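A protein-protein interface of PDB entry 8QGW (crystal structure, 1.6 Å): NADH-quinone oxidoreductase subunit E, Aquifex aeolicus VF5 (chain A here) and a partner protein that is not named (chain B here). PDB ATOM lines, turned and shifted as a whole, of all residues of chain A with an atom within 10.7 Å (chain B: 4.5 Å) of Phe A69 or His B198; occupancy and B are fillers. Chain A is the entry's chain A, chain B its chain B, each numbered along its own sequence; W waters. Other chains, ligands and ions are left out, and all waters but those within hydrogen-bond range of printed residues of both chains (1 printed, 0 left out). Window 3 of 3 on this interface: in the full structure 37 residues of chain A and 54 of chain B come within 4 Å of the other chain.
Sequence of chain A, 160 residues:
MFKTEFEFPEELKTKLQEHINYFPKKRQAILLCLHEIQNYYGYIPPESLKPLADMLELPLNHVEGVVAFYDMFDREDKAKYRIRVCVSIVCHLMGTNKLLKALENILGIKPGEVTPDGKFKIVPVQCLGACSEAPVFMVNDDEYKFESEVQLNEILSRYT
The side-chain hydroxyl of Tyr A70 sits at hydrogen-bond distance from the backbone NH of Gly B197 (3.3 Å).
Gly A65 touches Arg B196. Phe A69 touches Ala B179. Phe A69 touches Ile B181. CB of Phe A69 touches CG of Arg B196, at 3.7 Å. Phe A69 touches Gly B197 (CZ to O, 3.4 Å). Phe A69 touches His B198. Tyr A70 touches Arg B196.
Of chain B, only Ala B179, Ile B181, Arg B196, Gly B197 and His B198 come within 4 Å of Phe A69. His B198 touches just one residue of chain A: Phe A69. Ala B179 touches one residue of chain A. No residue of chain A comes within 4 Å of Ala B187. Of the printed residues of chain A, Gly B197 touches Phe A69 and Tyr A70. No residue of chain A comes within 4 Å of Pro B199. Printed residues of chain A within 4 Å of Arg B196: Gly A65, Phe A69 and Tyr A70. Printed residues of chain A within 4 Å of Ile B181: Phe A69. Printed residues of chain B within 4 Å of Tyr A70: Arg B196 (3.7 Å) and Gly B197 (3.3 Å). Printed residues of chain B within 4 Å of Gly A65: Arg B196 (3.6 Å). Asn A61 touches none of the printed residues of chain B. Arg A75 touches none of the printed residues of chain B. The nearest residue of chain A that does not touch His B198 is Tyr A70 (6.2 Å).
Printed residues of chain A that touch a printed residue of chain B: Gly A65, Phe A69 and Tyr A70. Along chain A the printed residues that touch a printed residue of chain B span positions 65 to 70. Hydrophobic or aromatic side chains of chain B within 4 Å of the printed part of chain A: Ala B179, Ile B181 and His B198. Along chain B the printed residues that touch a printed residue of chain A span positions 179 to 198. Among the printed residues, 8 pairs touch across the chains.
Water W1 bridges the backbone carbonyl oxygen of Gly A65 and the guanidinium group of Arg B196.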
ATOM      1  N   ILE A  30       2.658  -6.188 -17.743  1.00  0.00           N
ATOM      2  CA  ILE A  30       3.413  -7.199 -17.010  1.00  0.00           C
ATOM      3  C   ILE A  30       2.735  -8.568 -17.026  1.00  0.00           C
ATOM      4  O   ILE A  30       3.417  -9.566 -17.217  1.00  0.00           O
ATOM      5  CB  ILE A  30       3.700  -6.734 -15.570  1.00  0.00           C
ATOM      6  CG1 ILE A  30       4.595  -7.736 -14.837  1.00  0.00           C
ATOM      7  CG2 ILE A  30       2.414  -6.447 -14.798  1.00  0.00           C
ATOM      8  CD1 ILE A  30       5.271  -7.159 -13.615  1.00  0.00           C
ATOM      9  N   LEU A  31       1.425  -8.638 -16.766  1.00  0.00           N
ATOM     10  CA  LEU A  31       0.741  -9.932 -16.733  1.00  0.00           C
ATOM     11  C   LEU A  31       0.622 -10.561 -18.122  1.00  0.00           C
ATOM     12  O   LEU A  31       0.754 -11.782 -18.241  1.00  0.00           O
ATOM     13  CB  LEU A  31      -0.644  -9.788 -16.097  1.00  0.00           C
ATOM     14  CG  LEU A  31      -0.622  -9.252 -14.667  1.00  0.00           C
ATOM     15  CD1 LEU A  31      -1.996  -9.270 -14.040  1.00  0.00           C
ATOM     16  CD2 LEU A  31       0.360 -10.020 -13.794  1.00  0.00           C
ATOM     17  N   LEU A  34       3.928 -12.085 -18.778  1.00  0.00           N
ATOM     18  CA  LEU A  34       4.130 -13.301 -17.997  1.00  0.00           C
ATOM     19  C   LEU A  34       3.293 -14.464 -18.534  1.00  0.00           C
ATOM     20  O   LEU A  34       3.771 -15.598 -18.593  1.00  0.00           O
ATOM     21  CB  LEU A  34       3.835 -12.991 -16.532  1.00  0.00           C
ATOM     22  CG  LEU A  34       4.902 -12.135 -15.858  1.00  0.00           C
ATOM     23  CD1 LEU A  34       4.443 -11.735 -14.485  1.00  0.00           C
ATOM     24  CD2 LEU A  34       6.242 -12.857 -15.780  1.00  0.00           C
ATOM     25  N   ILE A  44       7.326 -20.286 -15.922  1.00  0.00           N
ATOM     26  CA  ILE A  44       8.122 -19.067 -15.881  1.00  0.00           C
ATOM     27  C   ILE A  44       9.556 -19.416 -15.491  1.00  0.00           C
ATOM     28  O   ILE A  44       9.821 -19.681 -14.324  1.00  0.00           O
ATOM     29  CB  ILE A  44       7.531 -18.038 -14.892  1.00  0.00           C
ATOM     30  CG1 ILE A  44       6.058 -17.708 -15.166  1.00  0.00           C
ATOM     31  CG2 ILE A  44       8.397 -16.782 -14.878  1.00  0.00           C
ATOM     32  CD1 ILE A  44       5.842 -16.925 -16.442  1.00  0.00           C
ATOM     33  N   LEU A  49      12.903 -13.451 -15.727  1.00  0.00           N
ATOM     34  CA  LEU A  49      12.360 -12.292 -15.022  1.00  0.00           C
ATOM     35  C   LEU A  49      13.236 -11.045 -15.148  1.00  0.00           C
ATOM     36  O   LEU A  49      12.693  -9.951 -15.298  1.00  0.00           O
ATOM     37  CB  LEU A  49      12.164 -12.659 -13.549  1.00  0.00           C
ATOM     38  CG  LEU A  49      11.165 -13.789 -13.331  1.00  0.00           C
ATOM     39  CD1 LEU A  49      10.734 -13.855 -11.887  1.00  0.00           C
ATOM     40  CD2 LEU A  49       9.961 -13.614 -14.241  1.00  0.00           C
ATOM     41  N   ASN A  61      12.845  -7.004  -8.340  1.00  0.00           N
ATOM     42  CA  ASN A  61      12.090  -7.478  -7.181  1.00  0.00           C
ATOM     43  C   ASN A  61      10.602  -7.186  -7.355  1.00  0.00           C
ATOM     44  O   ASN A  61       9.798  -7.934  -6.819  1.00  0.00           O
ATOM     45  CB  ASN A  61      12.615  -6.988  -5.825  1.00  0.00           C
ATOM     46  CG  ASN A  61      12.709  -5.482  -5.691  1.00  0.00           C
ATOM     47  OD1 ASN A  61      12.003  -4.743  -6.374  1.00  0.00           O
ATOM     48  ND2 ASN A  61      13.577  -5.017  -4.805  1.00  0.00           N
ATOM     49  N   HIS A  62      10.245  -6.119  -8.096  1.00  0.00           N
ATOM     50  CA  HIS A  62       8.852  -5.860  -8.455  1.00  0.00           C
ATOM     51  C   HIS A  62       8.303  -7.012  -9.292  1.00  0.00           C
ATOM     52  O   HIS A  62       7.227  -7.532  -9.013  1.00  0.00           O
ATOM     53  CB  HIS A  62       8.715  -4.530  -9.210  1.00  0.00           C
ATOM     54  CG  HIS A  62       7.321  -4.160  -9.612  1.00  0.00           C
ATOM     55  ND1 HIS A  62       6.874  -2.863  -9.507  1.00  0.00           N
ATOM     56  CD2 HIS A  62       6.316  -4.864 -10.165  1.00  0.00           C
ATOM     57  CE1 HIS A  62       5.621  -2.815  -9.948  1.00  0.00           C
ATOM     58  NE2 HIS A  62       5.265  -4.015 -10.352  1.00  0.00           N
ATOM     59  N   VAL A  63       9.016  -7.386 -10.357  1.00  0.00           N
ATOM     60  CA  VAL A  63       8.550  -8.475 -11.201  1.00  0.00           C
ATOM     61  C   VAL A  63       8.452  -9.764 -10.375  1.00  0.00           C
ATOM     62  O   VAL A  63       7.476 -10.500 -10.485  1.00  0.00           O
ATOM     63  CB  VAL A  63       9.431  -8.644 -12.452  1.00  0.00           C
ATOM     64  CG1 VAL A  63       8.983  -9.833 -13.294  1.00  0.00           C
ATOM     65  CG2 VAL A  63       9.481  -7.360 -13.277  1.00  0.00           C
ATOM     66  N   GLU A  64       9.462 -10.046  -9.542  1.00  0.00           N
ATOM     67  CA  GLU A  64       9.472 -11.306  -8.811  1.00  0.00           C
ATOM     68  C   GLU A  64       8.248 -11.362  -7.896  1.00  0.00           C
ATOM     69  O   GLU A  64       7.620 -12.404  -7.773  1.00  0.00           O
ATOM     70  CB  GLU A  64      10.758 -11.471  -8.003  1.00  0.00           C
ATOM     71  CG  GLU A  64      11.987 -11.784  -8.850  1.00  0.00           C
ATOM     72  CD  GLU A  64      13.306 -11.674  -8.106  1.00  0.00           C
ATOM     73  OE1 GLU A  64      13.366 -10.934  -7.088  1.00  0.00           O
ATOM     74  OE2 GLU A  64      14.294 -12.307  -8.555  1.00  0.00           O
ATOM     75  N   GLY A  65       7.925 -10.234  -7.246  1.00  0.00           N
ATOM     76  CA  GLY A  65       6.776 -10.162  -6.354  1.00  0.00           C
ATOM     77  C   GLY A  65       5.464 -10.434  -7.084  1.00  0.00           C
ATOM     78  O   GLY A  65       4.566 -11.106  -6.583  1.00  0.00           O
ATOM     79  N   VAL A  66       5.363  -9.934  -8.317  1.00  0.00           N
ATOM     80  CA  VAL A  66       4.167 -10.135  -9.110  1.00  0.00           C
ATOM     81  C   VAL A  66       4.030 -11.607  -9.490  1.00  0.00           C
ATOM     82  O   VAL A  66       2.945 -12.181  -9.386  1.00  0.00           O
ATOM     83  CB  VAL A  66       4.126  -9.176 -10.312  1.00  0.00           C
ATOM     84  CG1 VAL A  66       3.190  -9.652 -11.412  1.00  0.00           C
ATOM     85  CG2 VAL A  66       3.788  -7.768  -9.852  1.00  0.00           C
ATOM     86  N   VAL A  67       5.127 -12.245  -9.915  1.00  0.00           N
ATOM     87  CA  VAL A  67       5.030 -13.652 -10.274  1.00  0.00           C
ATOM     88  C   VAL A  67       4.573 -14.460  -9.056  1.00  0.00           C
ATOM     89  O   VAL A  67       3.779 -15.384  -9.195  1.00  0.00           O
ATOM     90  CB  VAL A  67       6.344 -14.203 -10.857  1.00  0.00           C
ATOM     91  CG1 VAL A  67       6.280 -15.713 -11.049  1.00  0.00           C
ATOM     92  CG2 VAL A  67       6.721 -13.530 -12.163  1.00  0.00           C
ATOM     93  N   ALA A  68       5.082 -14.109  -7.864  1.00  0.00           N
ATOM     94  CA  ALA A  68       4.786 -14.846  -6.646  1.00  0.00           C
ATOM     95  C   ALA A  68       3.315 -14.694  -6.284  1.00  0.00           C
ATOM     96  O   ALA A  68       2.699 -15.625  -5.771  1.00  0.00           O
ATOM     97  CB  ALA A  68       5.681 -14.371  -5.513  1.00  0.00           C
ATOM     98  N   PHE A  69       2.759 -13.516  -6.588  1.00  0.00           N
ATOM     99  CA  PHE A  69       1.424 -13.161  -6.130  1.00  0.00           C
ATOM    100  C   PHE A  69       0.326 -13.894  -6.896  1.00  0.00           C
ATOM    101  O   PHE A  69      -0.709 -14.239  -6.313  1.00  0.00           O
ATOM    102  CB  PHE A  69       1.195 -11.650  -6.232  1.00  0.00           C
ATOM    103  CG  PHE A  69      -0.169 -11.212  -5.766  1.00  0.00           C
ATOM    104  CD1 PHE A  69      -0.412 -10.966  -4.420  1.00  0.00           C
ATOM    105  CD2 PHE A  69      -1.204 -11.049  -6.676  1.00  0.00           C
ATOM    106  CE1 PHE A  69      -1.681 -10.571  -4.007  1.00  0.00           C
ATOM    107  CE2 PHE A  69      -2.471 -10.673  -6.256  1.00  0.00           C
ATOM    108  CZ  PHE A  69      -2.706 -10.445  -4.920  1.00  0.00           C
ATOM    109  N   TYR A  70       0.534 -14.048  -8.211  1.00  0.00           N
ATOM    110  CA  TYR A  70      -0.512 -14.464  -9.133  1.00  0.00           C
ATOM    111  C   TYR A  70      -0.426 -15.975  -9.354  1.00  0.00           C
ATOM    112  O   TYR A  70       0.567 -16.484  -9.864  1.00  0.00           O
ATOM    113  CB  TYR A  70      -0.435 -13.634 -10.418  1.00  0.00           C
ATOM    114  CG  TYR A  70      -0.894 -12.205 -10.278  1.00  0.00           C
ATOM    115  CD1 TYR A  70      -2.240 -11.874 -10.216  1.00  0.00           C
ATOM    116  CD2 TYR A  70       0.013 -11.169 -10.168  1.00  0.00           C
ATOM    117  CE1 TYR A  70      -2.650 -10.557 -10.099  1.00  0.00           C
ATOM    118  CE2 TYR A  70      -0.381  -9.849 -10.041  1.00  0.00           C
ATOM    119  CZ  TYR A  70      -1.725  -9.536  -9.995  1.00  0.00           C
ATOM    120  OH  TYR A  70      -2.107  -8.220  -9.840  1.00  0.00           O
ATOM    121  N   ASP A  71      -1.498 -16.674  -8.963  1.00  0.00           N
ATOM    122  CA  ASP A  71      -1.502 -18.128  -8.844  1.00  0.00           C
ATOM    123  C   ASP A  71      -1.414 -18.860 -10.185  1.00  0.00           C
ATOM    124  O   ASP A  71      -1.018 -20.025 -10.197  1.00  0.00           O
ATOM    125  CB  ASP A  71      -2.762 -18.633  -8.138  1.00  0.00           C
ATOM    126  CG  ASP A  71      -2.736 -18.485  -6.626  1.00  0.00           C
ATOM    127  OD1 ASP A  71      -1.681 -18.116  -6.078  1.00  0.00           O
ATOM    128  OD2 ASP A  71      -3.790 -18.742  -6.000  1.00  0.00           O
ATOM    129  N   MET A  72      -1.748 -18.221 -11.312  1.00  0.00           N
ATOM    130  CA  MET A  72      -1.684 -18.941 -12.580  1.00  0.00           C
ATOM    131  C   MET A  72      -0.229 -19.218 -12.956  1.00  0.00           C
ATOM    132  O   MET A  72       0.065 -20.190 -13.667  1.00  0.00           O
ATOM    133  CB  MET A  72      -2.361 -18.169 -13.714  1.00  0.00           C
ATOM    134  CG  MET A  72      -3.879 -18.238 -13.635  1.00  0.00           C
ATOM    135  SD  MET A  72      -4.747 -17.453 -15.016  1.00  0.00           S
ATOM    136  CE  MET A  72      -4.386 -18.583 -16.347  1.00  0.00           C
ATOM    137  N   PHE A  73       0.701 -18.374 -12.475  1.00  0.00           N
ATOM    138  CA  PHE A  73       2.092 -18.502 -12.884  1.00  0.00           C
ATOM    139  C   PHE A  73       2.812 -19.571 -12.061  1.00  0.00           C
ATOM    140  O   PHE A  73       2.652 -19.658 -10.845  1.00  0.00           O
ATOM    141  CB  PHE A  73       2.803 -17.150 -12.789  1.00  0.00           C
ATOM    142  CG  PHE A  73       2.150 -16.052 -13.593  1.00  0.00           C
ATOM    143  CD1 PHE A  73       1.742 -16.269 -14.909  1.00  0.00           C
ATOM    144  CD2 PHE A  73       1.955 -14.795 -13.049  1.00  0.00           C
ATOM    145  CE1 PHE A  73       1.147 -15.261 -15.652  1.00  0.00           C
ATOM    146  CE2 PHE A  73       1.366 -13.787 -13.800  1.00  0.00           C
ATOM    147  CZ  PHE A  73       0.956 -14.023 -15.092  1.00  0.00           C
ATOM    148  N   ASP A  74       3.682 -20.333 -12.730  1.00  0.00           N
ATOM    149  CA  ASP A  74       4.397 -21.460 -12.132  1.00  0.00           C
ATOM    150  C   ASP A  74       5.878 -21.337 -12.484  1.00  0.00           C
ATOM    151  O   ASP A  74       6.227 -21.410 -13.655  1.00  0.00           O
ATOM    152  CB  ASP A  74       3.784 -22.765 -12.654  1.00  0.00           C
ATOM    153  CG  ASP A  74       4.342 -24.077 -12.128  1.00  0.00           C
ATOM    154  OD1 ASP A  74       5.362 -24.052 -11.401  1.00  0.00           O
ATOM    155  OD2 ASP A  74       3.718 -25.137 -12.442  1.00  0.00           O
ATOM    156  N   ARG A  75       6.735 -21.153 -11.471  1.00  0.00           N
ATOM    157  CA  ARG A  75       8.177 -21.070 -11.678  1.00  0.00           C
ATOM    158  C   ARG A  75       8.873 -22.408 -11.435  1.00  0.00           C
ATOM    159  O   ARG A  75      10.071 -22.507 -11.658  1.00  0.00           O
ATOM    160  CB  ARG A  75       8.803 -20.044 -10.728  1.00  0.00           C
ATOM    161  CG  ARG A  75       8.677 -18.602 -11.194  1.00  0.00           C
ATOM    162  CD  ARG A  75       9.356 -17.660 -10.218  1.00  0.00           C
ATOM    163  NE  ARG A  75       8.589 -17.488  -8.994  1.00  0.00           N
ATOM    164  CZ  ARG A  75       8.848 -16.562  -8.071  1.00  0.00           C
ATOM    165  NH1 ARG A  75       9.908 -15.779  -8.188  1.00  0.00           N
ATOM    166  NH2 ARG A  75       8.042 -16.426  -7.034  1.00  0.00           N
ATOM    167  N   ALA B 179      -6.030 -14.291  -9.210  1.00  0.00           N
ATOM    168  CA  ALA B 179      -6.367 -13.762  -7.892  1.00  0.00           C
ATOM    169  C   ALA B 179      -7.806 -13.260  -7.857  1.00  0.00           C
ATOM    170  O   ALA B 179      -8.135 -12.310  -8.556  1.00  0.00           O
ATOM    171  CB  ALA B 179      -5.394 -12.658  -7.561  1.00  0.00           C
ATOM    172  N   ILE B 181      -9.063 -11.587  -5.575  1.00  0.00           N
ATOM    173  CA  ILE B 181      -9.083 -10.267  -4.953  1.00  0.00           C
ATOM    174  C   ILE B 181      -8.982  -9.188  -6.035  1.00  0.00           C
ATOM    175  O   ILE B 181      -9.358  -8.050  -5.794  1.00  0.00           O
ATOM    176  CB  ILE B 181      -7.991 -10.105  -3.875  1.00  0.00           C
ATOM    177  CG1 ILE B 181      -8.204  -8.858  -3.015  1.00  0.00           C
ATOM    178  CG2 ILE B 181      -6.595 -10.104  -4.471  1.00  0.00           C
ATOM    179  CD1 ILE B 181      -9.557  -8.816  -2.337  1.00  0.00           C
ATOM    180  N   THR B 186     -10.376  -1.689  -6.181  1.00  0.00           N
ATOM    181  CA  THR B 186      -9.095  -1.012  -5.978  1.00  0.00           C
ATOM    182  C   THR B 186      -7.912  -1.952  -6.215  1.00  0.00           C
ATOM    183  O   THR B 186      -6.870  -1.522  -6.744  1.00  0.00           O
ATOM    184  CB  THR B 186      -8.999  -0.307  -4.623  1.00  0.00           C
ATOM    185  OG1 THR B 186      -9.013  -1.258  -3.565  1.00  0.00           O
ATOM    186  CG2 THR B 186     -10.140   0.674  -4.424  1.00  0.00           C
ATOM    187  N   ALA B 187      -8.072  -3.246  -5.907  1.00  0.00           N
ATOM    188  CA  ALA B 187      -7.047  -4.225  -6.258  1.00  0.00           C
ATOM    189  C   ALA B 187      -6.959  -4.377  -7.784  1.00  0.00           C
ATOM    190  O   ALA B 187      -5.876  -4.523  -8.356  1.00  0.00           O
ATOM    191  CB  ALA B 187      -7.334  -5.533  -5.581  1.00  0.00           C
ATOM    192  N   GLU B 190      -4.897  -1.540  -8.989  1.00  0.00           N
ATOM    193  CA  GLU B 190      -3.490  -1.812  -8.727  1.00  0.00           C
ATOM    194  C   GLU B 190      -2.923  -2.774  -9.774  1.00  0.00           C
ATOM    195  O   GLU B 190      -1.795  -2.610 -10.256  1.00  0.00           O
ATOM    196  CB  GLU B 190      -3.288  -2.396  -7.335  1.00  0.00           C
ATOM    197  CG  GLU B 190      -3.508  -1.382  -6.231  1.00  0.00           C
ATOM    198  CD  GLU B 190      -2.401  -0.342  -6.126  1.00  0.00           C
ATOM    199  OE1 GLU B 190      -2.714   0.836  -6.178  1.00  0.00           O
ATOM    200  OE2 GLU B 190      -1.217  -0.721  -6.044  1.00  0.00           O
ATOM    201  N   ARG B 196       0.904  -5.966  -7.717  1.00  0.00           N
ATOM    202  CA  ARG B 196       0.116  -6.967  -7.025  1.00  0.00           C
ATOM    203  C   ARG B 196      -1.281  -6.412  -6.744  1.00  0.00           C
ATOM    204  O   ARG B 196      -1.443  -5.213  -6.568  1.00  0.00           O
ATOM    205  CB  ARG B 196       0.836  -7.365  -5.737  1.00  0.00           C
ATOM    206  CG  ARG B 196       2.170  -8.044  -6.017  1.00  0.00           C
ATOM    207  CD  ARG B 196       2.897  -8.465  -4.755  1.00  0.00           C
ATOM    208  NE  ARG B 196       3.268  -7.328  -3.947  1.00  0.00           N
ATOM    209  CZ  ARG B 196       3.970  -7.418  -2.821  1.00  0.00           C
ATOM    210  NH1 ARG B 196       4.189  -6.351  -2.074  1.00  0.00           N
ATOM    211  NH2 ARG B 196       4.426  -8.595  -2.431  1.00  0.00           N
ATOM    212  N   GLY B 197      -2.253  -7.319  -6.666  1.00  0.00           N
ATOM    213  CA  GLY B 197      -3.643  -6.972  -6.408  1.00  0.00           C
ATOM    214  C   GLY B 197      -3.908  -6.754  -4.922  1.00  0.00           C
ATOM    215  O   GLY B 197      -4.432  -7.635  -4.242  1.00  0.00           O
ATOM    216  N   HIS B 198      -3.459  -5.605  -4.403  1.00  0.00           N
ATOM    217  CA  HIS B 198      -3.676  -5.248  -3.014  1.00  0.00           C
ATOM    218  C   HIS B 198      -4.708  -4.129  -2.944  1.00  0.00           C
ATOM    219  O   HIS B 198      -4.438  -3.006  -3.390  1.00  0.00           O
ATOM    220  CB  HIS B 198      -2.374  -4.783  -2.364  1.00  0.00           C
ATOM    221  CG  HIS B 198      -1.427  -5.893  -2.082  1.00  0.00           C
ATOM    222  ND1 HIS B 198      -0.110  -5.660  -1.753  1.00  0.00           N
ATOM    223  CD2 HIS B 198      -1.566  -7.222  -2.100  1.00  0.00           C
ATOM    224  CE1 HIS B 198       0.502  -6.830  -1.578  1.00  0.00           C
ATOM    225  NE2 HIS B 198      -0.348  -7.785  -1.799  1.00  0.00           N
ATOM    226  N   PRO B 199      -5.895  -4.375  -2.352  1.00  0.00           N
ATOM    227  CA  PRO B 199      -6.869  -3.308  -2.139  1.00  0.00           C
ATOM    228  C   PRO B 199      -6.283  -2.100  -1.414  1.00  0.00           C
ATOM    229  O   PRO B 199      -5.370  -2.232  -0.598  1.00  0.00           O
ATOM    230  CB  PRO B 199      -7.954  -3.955  -1.265  1.00  0.00           C
ATOM    231  CG  PRO B 199      -7.885  -5.421  -1.670  1.00  0.00           C
ATOM    232  CD  PRO B 199      -6.401  -5.682  -1.885  1.00  0.00           C
ATOM    233  N   ARG B 200      -6.838  -0.934  -1.749  1.00  0.00           N
ATOM    234  CA  ARG B 200      -6.477   0.335  -1.152  1.00  0.00           C
ATOM    235  C   ARG B 200      -7.530   0.667  -0.094  1.00  0.00           C
ATOM    236  O   ARG B 200      -8.708   0.356  -0.273  1.00  0.00           O
ATOM    237  CB  ARG B 200      -6.485   1.450  -2.216  1.00  0.00           C
ATOM    238  CG  ARG B 200      -5.559   1.239  -3.418  1.00  0.00           C
ATOM    239  CD  ARG B 200      -5.757   2.356  -4.437  1.00  0.00           C
ATOM    240  NE  ARG B 200      -4.918   2.299  -5.634  1.00  0.00           N
ATOM    241  CZ  ARG B 200      -5.021   3.129  -6.680  1.00  0.00           C
ATOM    242  NH1 ARG B 200      -4.148   3.062  -7.680  1.00  0.00           N
ATOM    243  NH2 ARG B 200      -5.957   4.069  -6.689  1.00  0.00           N
ATOM    244  N   CYS B 347      -5.520 -11.574   0.454  1.00  0.00           N
ATOM    245  CA  CYS B 347      -4.280 -11.004  -0.059  1.00  0.00           C
ATOM    246  C   CYS B 347      -3.200 -10.845   1.021  1.00  0.00           C
ATOM    247  O   CYS B 347      -2.024 -10.628   0.691  1.00  0.00           O
ATOM    248  CB  CYS B 347      -4.494  -9.676  -0.789  1.00  0.00           C
ATOM    249  SG  CYS B 347      -4.665  -8.224   0.275  1.00  0.00           S
ATOM    250  N   GLN B 349      -2.705  -8.514   3.455  1.00  0.00           N
ATOM    251  CA  GLN B 349      -2.304  -7.196   3.951  1.00  0.00           C
ATOM    252  C   GLN B 349      -2.748  -6.969   5.391  1.00  0.00           C
ATOM    253  O   GLN B 349      -2.078  -6.256   6.140  1.00  0.00           O
ATOM    254  CB  GLN B 349      -2.921  -6.035   3.148  1.00  0.00           C
ATOM    255  CG  GLN B 349      -2.336  -5.772   1.779  1.00  0.00           C
ATOM    256  CD  GLN B 349      -2.981  -4.499   1.274  1.00  0.00           C
ATOM    257  OE1 GLN B 349      -2.463  -3.397   1.503  1.00  0.00           O
ATOM    258  NE2 GLN B 349      -4.173  -4.635   0.693  1.00  0.00           N
HETATM  259  O   HOH W   1       4.251 -11.311  -3.826  1.00  0.00           O
